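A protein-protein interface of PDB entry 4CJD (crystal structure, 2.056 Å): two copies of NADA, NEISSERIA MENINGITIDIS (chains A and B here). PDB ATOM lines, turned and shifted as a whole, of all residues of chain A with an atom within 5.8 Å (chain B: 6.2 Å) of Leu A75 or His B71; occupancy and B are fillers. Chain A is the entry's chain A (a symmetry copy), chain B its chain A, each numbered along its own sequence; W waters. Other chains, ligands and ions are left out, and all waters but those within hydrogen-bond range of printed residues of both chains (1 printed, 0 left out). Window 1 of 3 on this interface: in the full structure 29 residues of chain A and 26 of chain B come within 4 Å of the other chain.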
ATOM      1  N   LEU A  68      17.643 -13.242  17.734  1.00  0.00           N
ATOM      2  CA  LEU A  68      17.884 -14.672  17.974  1.00  0.00           C
ATOM      3  C   LEU A  68      19.212 -14.894  18.715  1.00  0.00           C
ATOM      4  O   LEU A  68      19.276 -15.729  19.630  1.00  0.00           O
ATOM      5  CB  LEU A  68      17.861 -15.461  16.668  1.00  0.00           C
ATOM      6  CG  LEU A  68      16.470 -15.779  16.108  1.00  0.00           C
ATOM      7  CD1 LEU A  68      16.581 -16.264  14.669  1.00  0.00           C
ATOM      8  CD2 LEU A  68      15.771 -16.803  16.956  1.00  0.00           C
ATOM      9  N   GLN A  70      20.627 -12.907  20.867  1.00  0.00           N
ATOM     10  CA  GLN A  70      20.369 -12.514  22.252  1.00  0.00           C
ATOM     11  C   GLN A  70      19.610 -13.589  22.991  1.00  0.00           C
ATOM     12  O   GLN A  70      19.862 -13.840  24.163  1.00  0.00           O
ATOM     13  CB  GLN A  70      19.564 -11.181  22.290  1.00  0.00           C
ATOM     14  CG  GLN A  70      20.427  -9.949  21.914  1.00  0.00           C
ATOM     15  CD  GLN A  70      19.653  -8.636  22.063  1.00  0.00           C
ATOM     16  OE1 GLN A  70      18.452  -8.632  22.368  1.00  0.00           O
ATOM     17  NE2 GLN A  70      20.349  -7.521  21.864  1.00  0.00           N
ATOM     18  N   HIS A  71      18.639 -14.208  22.322  1.00  0.00           N
ATOM     19  CA  HIS A  71      17.949 -15.367  22.905  1.00  0.00           C
ATOM     20  C   HIS A  71      18.857 -16.567  23.166  1.00  0.00           C
ATOM     21  O   HIS A  71      18.756 -17.184  24.214  1.00  0.00           O
ATOM     22  CB  HIS A  71      16.767 -15.744  22.028  1.00  0.00           C
ATOM     23  CG  HIS A  71      15.676 -14.736  22.122  1.00  0.00           C
ATOM     24  ND1 HIS A  71      14.454 -14.879  21.492  1.00  0.00           N
ATOM     25  CD2 HIS A  71      15.645 -13.524  22.745  1.00  0.00           C
ATOM     26  CE1 HIS A  71      13.695 -13.831  21.775  1.00  0.00           C
ATOM     27  NE2 HIS A  71      14.390 -12.996  22.541  1.00  0.00           N
ATOM     28  N   ASP A  72      19.779 -16.865  22.265  1.00  0.00           N
ATOM     29  CA  ASP A  72      20.803 -17.878  22.571  1.00  0.00           C
ATOM     30  C   ASP A  72      21.593 -17.606  23.851  1.00  0.00           C
ATOM     31  O   ASP A  72      21.783 -18.509  24.642  1.00  0.00           O
ATOM     32  CB  ASP A  72      21.819 -18.024  21.434  1.00  0.00           C
ATOM     33  CG  ASP A  72      21.328 -18.959  20.337  1.00  0.00           C
ATOM     34  OD1 ASP A  72      20.407 -19.771  20.609  1.00  0.00           O
ATOM     35  OD2 ASP A  72      21.867 -18.870  19.217  1.00  0.00           O
ATOM     36  N   GLN A  73      22.050 -16.367  24.034  1.00  0.00           N
ATOM     37  CA  GLN A  73      22.778 -15.976  25.232  1.00  0.00           C
ATOM     38  C   GLN A  73      21.870 -16.062  26.467  1.00  0.00           C
ATOM     39  O   GLN A  73      22.273 -16.595  27.474  1.00  0.00           O
ATOM     40  CB  GLN A  73      23.332 -14.542  25.081  1.00  0.00           C
ATOM     41  CG  GLN A  73      24.198 -14.084  26.265  1.00  0.00           C
ATOM     42  CD  GLN A  73      25.504 -14.880  26.359  1.00  0.00           C
ATOM     43  OE1 GLN A  73      26.297 -14.900  25.417  1.00  0.00           O
ATOM     44  NE2 GLN A  73      25.721 -15.549  27.492  1.00  0.00           N
ATOM     45  N   SER A  74      20.636 -15.557  26.381  1.00  0.00           N
ATOM     46  CA  SER A  74      19.705 -15.631  27.485  1.00  0.00           C
ATOM     47  C   SER A  74      19.457 -17.086  27.860  1.00  0.00           C
ATOM     48  O   SER A  74      19.438 -17.449  29.043  1.00  0.00           O
ATOM     49  CB  SER A  74      18.351 -14.926  27.125  1.00  0.00           C
ATOM     50  OG  SER A  74      18.584 -13.529  26.963  1.00  0.00           O
ATOM     51  N   LEU A  75      19.207 -17.914  26.857  1.00  0.00           N
ATOM     52  CA  LEU A  75      18.887 -19.304  27.165  1.00  0.00           C
ATOM     53  C   LEU A  75      20.041 -19.976  27.868  1.00  0.00           C
ATOM     54  O   LEU A  75      19.842 -20.695  28.853  1.00  0.00           O
ATOM     55  CB  LEU A  75      18.541 -20.103  25.911  1.00  0.00           C
ATOM     56  CG  LEU A  75      17.148 -19.914  25.324  1.00  0.00           C
ATOM     57  CD1 LEU A  75      17.077 -20.525  23.885  1.00  0.00           C
ATOM     58  CD2 LEU A  75      16.038 -20.453  26.265  1.00  0.00           C
ATOM     59  N   ALA A  76      21.243 -19.819  27.323  1.00  0.00           N
ATOM     60  CA  ALA A  76      22.403 -20.478  27.959  1.00  0.00           C
ATOM     61  C   ALA A  76      22.563 -19.967  29.404  1.00  0.00           C
ATOM     62  O   ALA A  76      22.763 -20.771  30.322  1.00  0.00           O
ATOM     63  CB  ALA A  76      23.704 -20.237  27.165  1.00  0.00           C
ATOM     64  N   ASP A  77      22.457 -18.645  29.614  1.00  0.00           N
ATOM     65  CA  ASP A  77      22.632 -18.107  30.977  1.00  0.00           C
ATOM     66  C   ASP A  77      21.564 -18.571  31.968  1.00  0.00           C
ATOM     67  O   ASP A  77      21.856 -18.912  33.108  1.00  0.00           O
ATOM     68  CB  ASP A  77      22.623 -16.574  30.968  1.00  0.00           C
ATOM     69  CG  ASP A  77      23.874 -16.006  30.327  1.00  0.00           C
ATOM     70  OD1 ASP A  77      24.888 -16.745  30.214  1.00  0.00           O
ATOM     71  OD2 ASP A  77      23.841 -14.843  29.917  1.00  0.00           O
ATOM     72  N   LEU A  78      20.320 -18.519  31.534  1.00  0.00           N
ATOM     73  CA  LEU A  78      19.223 -18.911  32.372  1.00  0.00           C
ATOM     74  C   LEU A  78      19.319 -20.410  32.672  1.00  0.00           C
ATOM     75  O   LEU A  78      19.036 -20.827  33.778  1.00  0.00           O
ATOM     76  CB  LEU A  78      17.891 -18.584  31.699  1.00  0.00           C
ATOM     77  CG  LEU A  78      16.678 -18.700  32.639  1.00  0.00           C
ATOM     78  CD1 LEU A  78      16.769 -17.801  33.928  1.00  0.00           C
ATOM     79  CD2 LEU A  78      15.394 -18.434  31.851  1.00  0.00           C
ATOM     80  N   THR A  79      19.702 -21.216  31.690  1.00  0.00           N
ATOM     81  CA  THR A  79      19.855 -22.651  31.977  1.00  0.00           C
ATOM     82  C   THR A  79      20.936 -22.862  33.022  1.00  0.00           C
ATOM     83  O   THR A  79      20.801 -23.730  33.872  1.00  0.00           O
ATOM     84  CB  THR A  79      20.203 -23.467  30.707  1.00  0.00           C
ATOM     85  OG1 THR A  79      19.233 -23.169  29.693  1.00  0.00           O
ATOM     86  CG2 THR A  79      20.236 -25.011  30.998  1.00  0.00           C
ATOM     87  N   GLY A  80      21.999 -22.052  32.976  1.00  0.00           N
ATOM     88  CA  GLY A  80      23.037 -22.156  33.998  1.00  0.00           C
ATOM     89  C   GLY A  80      22.518 -21.849  35.402  1.00  0.00           C
ATOM     90  O   GLY A  80      22.861 -22.538  36.354  1.00  0.00           O
ATOM     91  N   GLU B  66      14.513 -22.828  11.817  1.00  0.00           N
ATOM     92  CA  GLU B  66      15.014 -23.907  12.617  1.00  0.00           C
ATOM     93  C   GLU B  66      15.550 -23.436  13.965  1.00  0.00           C
ATOM     94  O   GLU B  66      15.410 -24.143  14.972  1.00  0.00           O
ATOM     95  CB  GLU B  66      16.116 -24.678  11.856  1.00  0.00           C
ATOM     96  CG  GLU B  66      16.688 -25.832  12.690  1.00  0.00           C
ATOM     97  CD  GLU B  66      15.628 -26.850  13.080  1.00  0.00           C
ATOM     98  OE1 GLU B  66      14.596 -26.920  12.395  1.00  0.00           O
ATOM     99  OE2 GLU B  66      15.802 -27.547  14.097  1.00  0.00           O
ATOM    100  N   VAL B  67      16.220 -22.279  14.011  1.00  0.00           N
ATOM    101  CA  VAL B  67      16.699 -21.814  15.325  1.00  0.00           C
ATOM    102  C   VAL B  67      15.472 -21.521  16.213  1.00  0.00           C
ATOM    103  O   VAL B  67      15.428 -21.866  17.429  1.00  0.00           O
ATOM    104  CB  VAL B  67      17.609 -20.529  15.204  1.00  0.00           C
ATOM    105  CG1 VAL B  67      18.027 -20.012  16.611  1.00  0.00           C
ATOM    106  CG2 VAL B  67      18.889 -20.856  14.370  1.00  0.00           C
ATOM    107  N   LEU B  68      14.464 -20.890  15.629  1.00  0.00           N
ATOM    108  CA  LEU B  68      13.258 -20.638  16.431  1.00  0.00           C
ATOM    109  C   LEU B  68      12.644 -21.953  16.939  1.00  0.00           C
ATOM    110  O   LEU B  68      12.217 -22.026  18.102  1.00  0.00           O
ATOM    111  CB  LEU B  68      12.227 -19.838  15.639  1.00  0.00           C
ATOM    112  CG  LEU B  68      12.488 -18.332  15.540  1.00  0.00           C
ATOM    113  CD1 LEU B  68      11.598 -17.713  14.471  1.00  0.00           C
ATOM    114  CD2 LEU B  68      12.266 -17.660  16.865  1.00  0.00           C
ATOM    115  N   ALA B  69      12.615 -23.007  16.109  1.00  0.00           N
ATOM    116  CA  ALA B  69      12.083 -24.306  16.593  1.00  0.00           C
ATOM    117  C   ALA B  69      12.899 -24.875  17.759  1.00  0.00           C
ATOM    118  O   ALA B  69      12.348 -25.483  18.699  1.00  0.00           O
ATOM    119  CB  ALA B  69      12.014 -25.374  15.447  1.00  0.00           C
ATOM    120  N   GLN B  70      14.216 -24.700  17.692  1.00  0.00           N
ATOM    121  CA  GLN B  70      15.089 -25.140  18.780  1.00  0.00           C
ATOM    122  C   GLN B  70      14.820 -24.358  20.043  1.00  0.00           C
ATOM    123  O   GLN B  70      14.852 -24.907  21.137  1.00  0.00           O
ATOM    124  CB  GLN B  70      16.581 -24.978  18.368  1.00  0.00           C
ATOM    125  CG  GLN B  70      17.037 -26.042  17.336  1.00  0.00           C
ATOM    126  CD  GLN B  70      18.532 -25.940  17.024  1.00  0.00           C
ATOM    127  OE1 GLN B  70      19.227 -25.034  17.508  1.00  0.00           O
ATOM    128  NE2 GLN B  70      19.031 -26.882  16.229  1.00  0.00           N
ATOM    129  N   HIS B  71      14.595 -23.053  19.906  1.00  0.00           N
ATOM    130  CA  HIS B  71      14.177 -22.240  21.056  1.00  0.00           C
ATOM    131  C   HIS B  71      12.832 -22.650  21.652  1.00  0.00           C
ATOM    132  O   HIS B  71      12.704 -22.713  22.865  1.00  0.00           O
ATOM    133  CB  HIS B  71      14.189 -20.771  20.667  1.00  0.00           C
ATOM    134  CG  HIS B  71      15.578 -20.263  20.501  1.00  0.00           C
ATOM    135  ND1 HIS B  71      15.876 -18.942  20.232  1.00  0.00           N
ATOM    136  CD2 HIS B  71      16.768 -20.928  20.516  1.00  0.00           C
ATOM    137  CE1 HIS B  71      17.191 -18.800  20.153  1.00  0.00           C
ATOM    138  NE2 HIS B  71      17.758 -19.989  20.329  1.00  0.00           N
ATOM    139  N   ASP B  72      11.855 -22.988  20.827  1.00  0.00           N
ATOM    140  CA  ASP B  72      10.618 -23.583  21.359  1.00  0.00           C
ATOM    141  C   ASP B  72      10.839 -24.827  22.219  1.00  0.00           C
ATOM    142  O   ASP B  72      10.254 -24.935  23.280  1.00  0.00           O
ATOM    143  CB  ASP B  72       9.645 -23.971  20.242  1.00  0.00           C
ATOM    144  CG  ASP B  72       8.793 -22.796  19.783  1.00  0.00           C
ATOM    145  OD1 ASP B  72       8.676 -21.805  20.548  1.00  0.00           O
ATOM    146  OD2 ASP B  72       8.253 -22.877  18.662  1.00  0.00           O
ATOM    147  N   GLN B  73      11.674 -25.753  21.748  1.00  0.00           N
ATOM    148  CA  GLN B  73      11.997 -26.960  22.495  1.00  0.00           C
ATOM    149  C   GLN B  73      12.759 -26.610  23.781  1.00  0.00           C
ATOM    150  O   GLN B  73      12.435 -27.119  24.829  1.00  0.00           O
ATOM    151  CB  GLN B  73      12.839 -27.921  21.626  1.00  0.00           C
ATOM    152  CG  GLN B  73      13.144 -29.266  22.306  1.00  0.00           C
ATOM    153  CD  GLN B  73      11.877 -30.105  22.505  1.00  0.00           C
ATOM    154  OE1 GLN B  73      11.178 -30.424  21.542  1.00  0.00           O
ATOM    155  NE2 GLN B  73      11.575 -30.450  23.757  1.00  0.00           N
ATOM    156  N   SER B  74      13.755 -25.724  23.705  1.00  0.00           N
ATOM    157  CA  SER B  74      14.497 -25.312  24.876  1.00  0.00           C
ATOM    158  C   SER B  74      13.555 -24.686  25.895  1.00  0.00           C
ATOM    159  O   SER B  74      13.633 -24.965  27.098  1.00  0.00           O
ATOM    160  CB  SER B  74      15.631 -24.300  24.492  1.00  0.00           C
ATOM    161  OG  SER B  74      16.599 -24.969  23.689  1.00  0.00           O
ATOM    162  N   LEU B  75      12.699 -23.789  25.427  1.00  0.00           N
ATOM    163  CA  LEU B  75      11.825 -23.102  26.371  1.00  0.00           C
ATOM    164  C   LEU B  75      10.922 -24.083  27.078  1.00  0.00           C
ATOM    165  O   LEU B  75      10.739 -24.002  28.297  1.00  0.00           O
ATOM    166  CB  LEU B  75      10.962 -22.043  25.687  1.00  0.00           C
ATOM    167  CG  LEU B  75      11.628 -20.717  25.340  1.00  0.00           C
ATOM    168  CD1 LEU B  75      10.726 -19.895  24.361  1.00  0.00           C
ATOM    169  CD2 LEU B  75      12.032 -19.916  26.606  1.00  0.00           C
ATOM    170  N   ALA B  76      10.284 -24.963  26.312  1.00  0.00           N
ATOM    171  CA  ALA B  76       9.369 -25.930  26.952  1.00  0.00           C
ATOM    172  C   ALA B  76      10.147 -26.790  27.965  1.00  0.00           C
ATOM    173  O   ALA B  76       9.678 -26.992  29.092  1.00  0.00           O
ATOM    174  CB  ALA B  76       8.673 -26.834  25.913  1.00  0.00           C
ATOM    175  N   LEU B  78      13.092 -26.221  29.599  1.00  0.00           N
ATOM    176  CA  LEU B  78      13.577 -25.449  30.708  1.00  0.00           C
ATOM    177  C   LEU B  78      12.404 -25.069  31.618  1.00  0.00           C
ATOM    178  O   LEU B  78      12.547 -25.077  32.825  1.00  0.00           O
ATOM    179  CB  LEU B  78      14.297 -24.196  30.213  1.00  0.00           C
ATOM    180  CG  LEU B  78      15.094 -23.467  31.309  1.00  0.00           C
ATOM    181  CD1 LEU B  78      16.175 -24.360  32.026  1.00  0.00           C
ATOM    182  CD2 LEU B  78      15.707 -22.190  30.732  1.00  0.00           C
HETATM  183  O   HOH W   1      13.904 -17.100  20.052  1.00  0.00           O
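A ring nitrogen (NE2) of His B71 sits at hydrogen-bond distance from the side-chain carboxylate of Asp A72.
The backbone carbonyl oxygen (O) of Leu A75 sits at hydrogen-bond distance from the side-chain hydroxyl (OG1) of Thr A79 (2.7 Å).
CG1 of Val B67 touches CD2 of Leu A68 (3.9 Å).
Leu A68 touches Leu B68.
O of Leu A68 touches CE1 of His B71, 3.7 Å away.
CE1 of His B71 touches CB of His A71 (3.6 Å).
CD1 of Leu A75 touches CD2 of His B71, at 3.4 Å.
Leu B78 touches Leu A78 (CD2 to CD2, 3.9 Å).
Thr A79 touches Leu B78.
Leu A75 touches one residue of chain B.
Of chain A, only Leu A68 (3.7 Å), His A71 (3.6 Å), Asp A72 (2.7 Å) and Leu A75 (3.4 Å) come within 4 Å of His B71.
Of the printed residues of chain A, Leu B78 touches Leu A78 and Thr A79.
Printed residues of chain A within 4 Å of Val B67: Leu A68.
Printed residues of chain B within 4 Å of Leu A68: Val B67, Leu B68 and His B71.
Printed residues of chain B within 4 Å of His A71: His B71.
Of the printed residues of chain B, Thr A79 touches Leu B78 (3.8 Å).
Gly A80 touches none of the printed residues of chain B.
The nearest residue of chain B that does not touch Leu A75 is Leu B75 (4.1 Å).
Of the 12 printed residues of chain B, 4 touch a printed residue of chain A.
Hydrophobic or aromatic side chains of chain B within 4 Å of the printed part of chain A: Val B67, Leu B68, His B71 and Leu B78.
Along chain B the printed residues that touch a printed residue of chain A span positions 67 to 78.
Leu A68 touches His B71, but with the chains exchanged His A71 does not touch Leu B68 (5.8 Å).
His A71 touches its own counterpart, His B71.
Leu A75 touches His B71, but with the chains exchanged His A71 does not touch Leu B75 (6.9 Å).
Leu A78 touches its own counterpart, Leu B78.
Of the 8 pairs that touch across the chains among the printed residues, 3 have their exchanged pair printed and touching as well.
Water W1 lies within hydrogen-bond range of a ring nitrogen (ND1) of His A71 (2.7 Å) and a ring nitrogen (ND1) of His B71 (2.7 Å).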
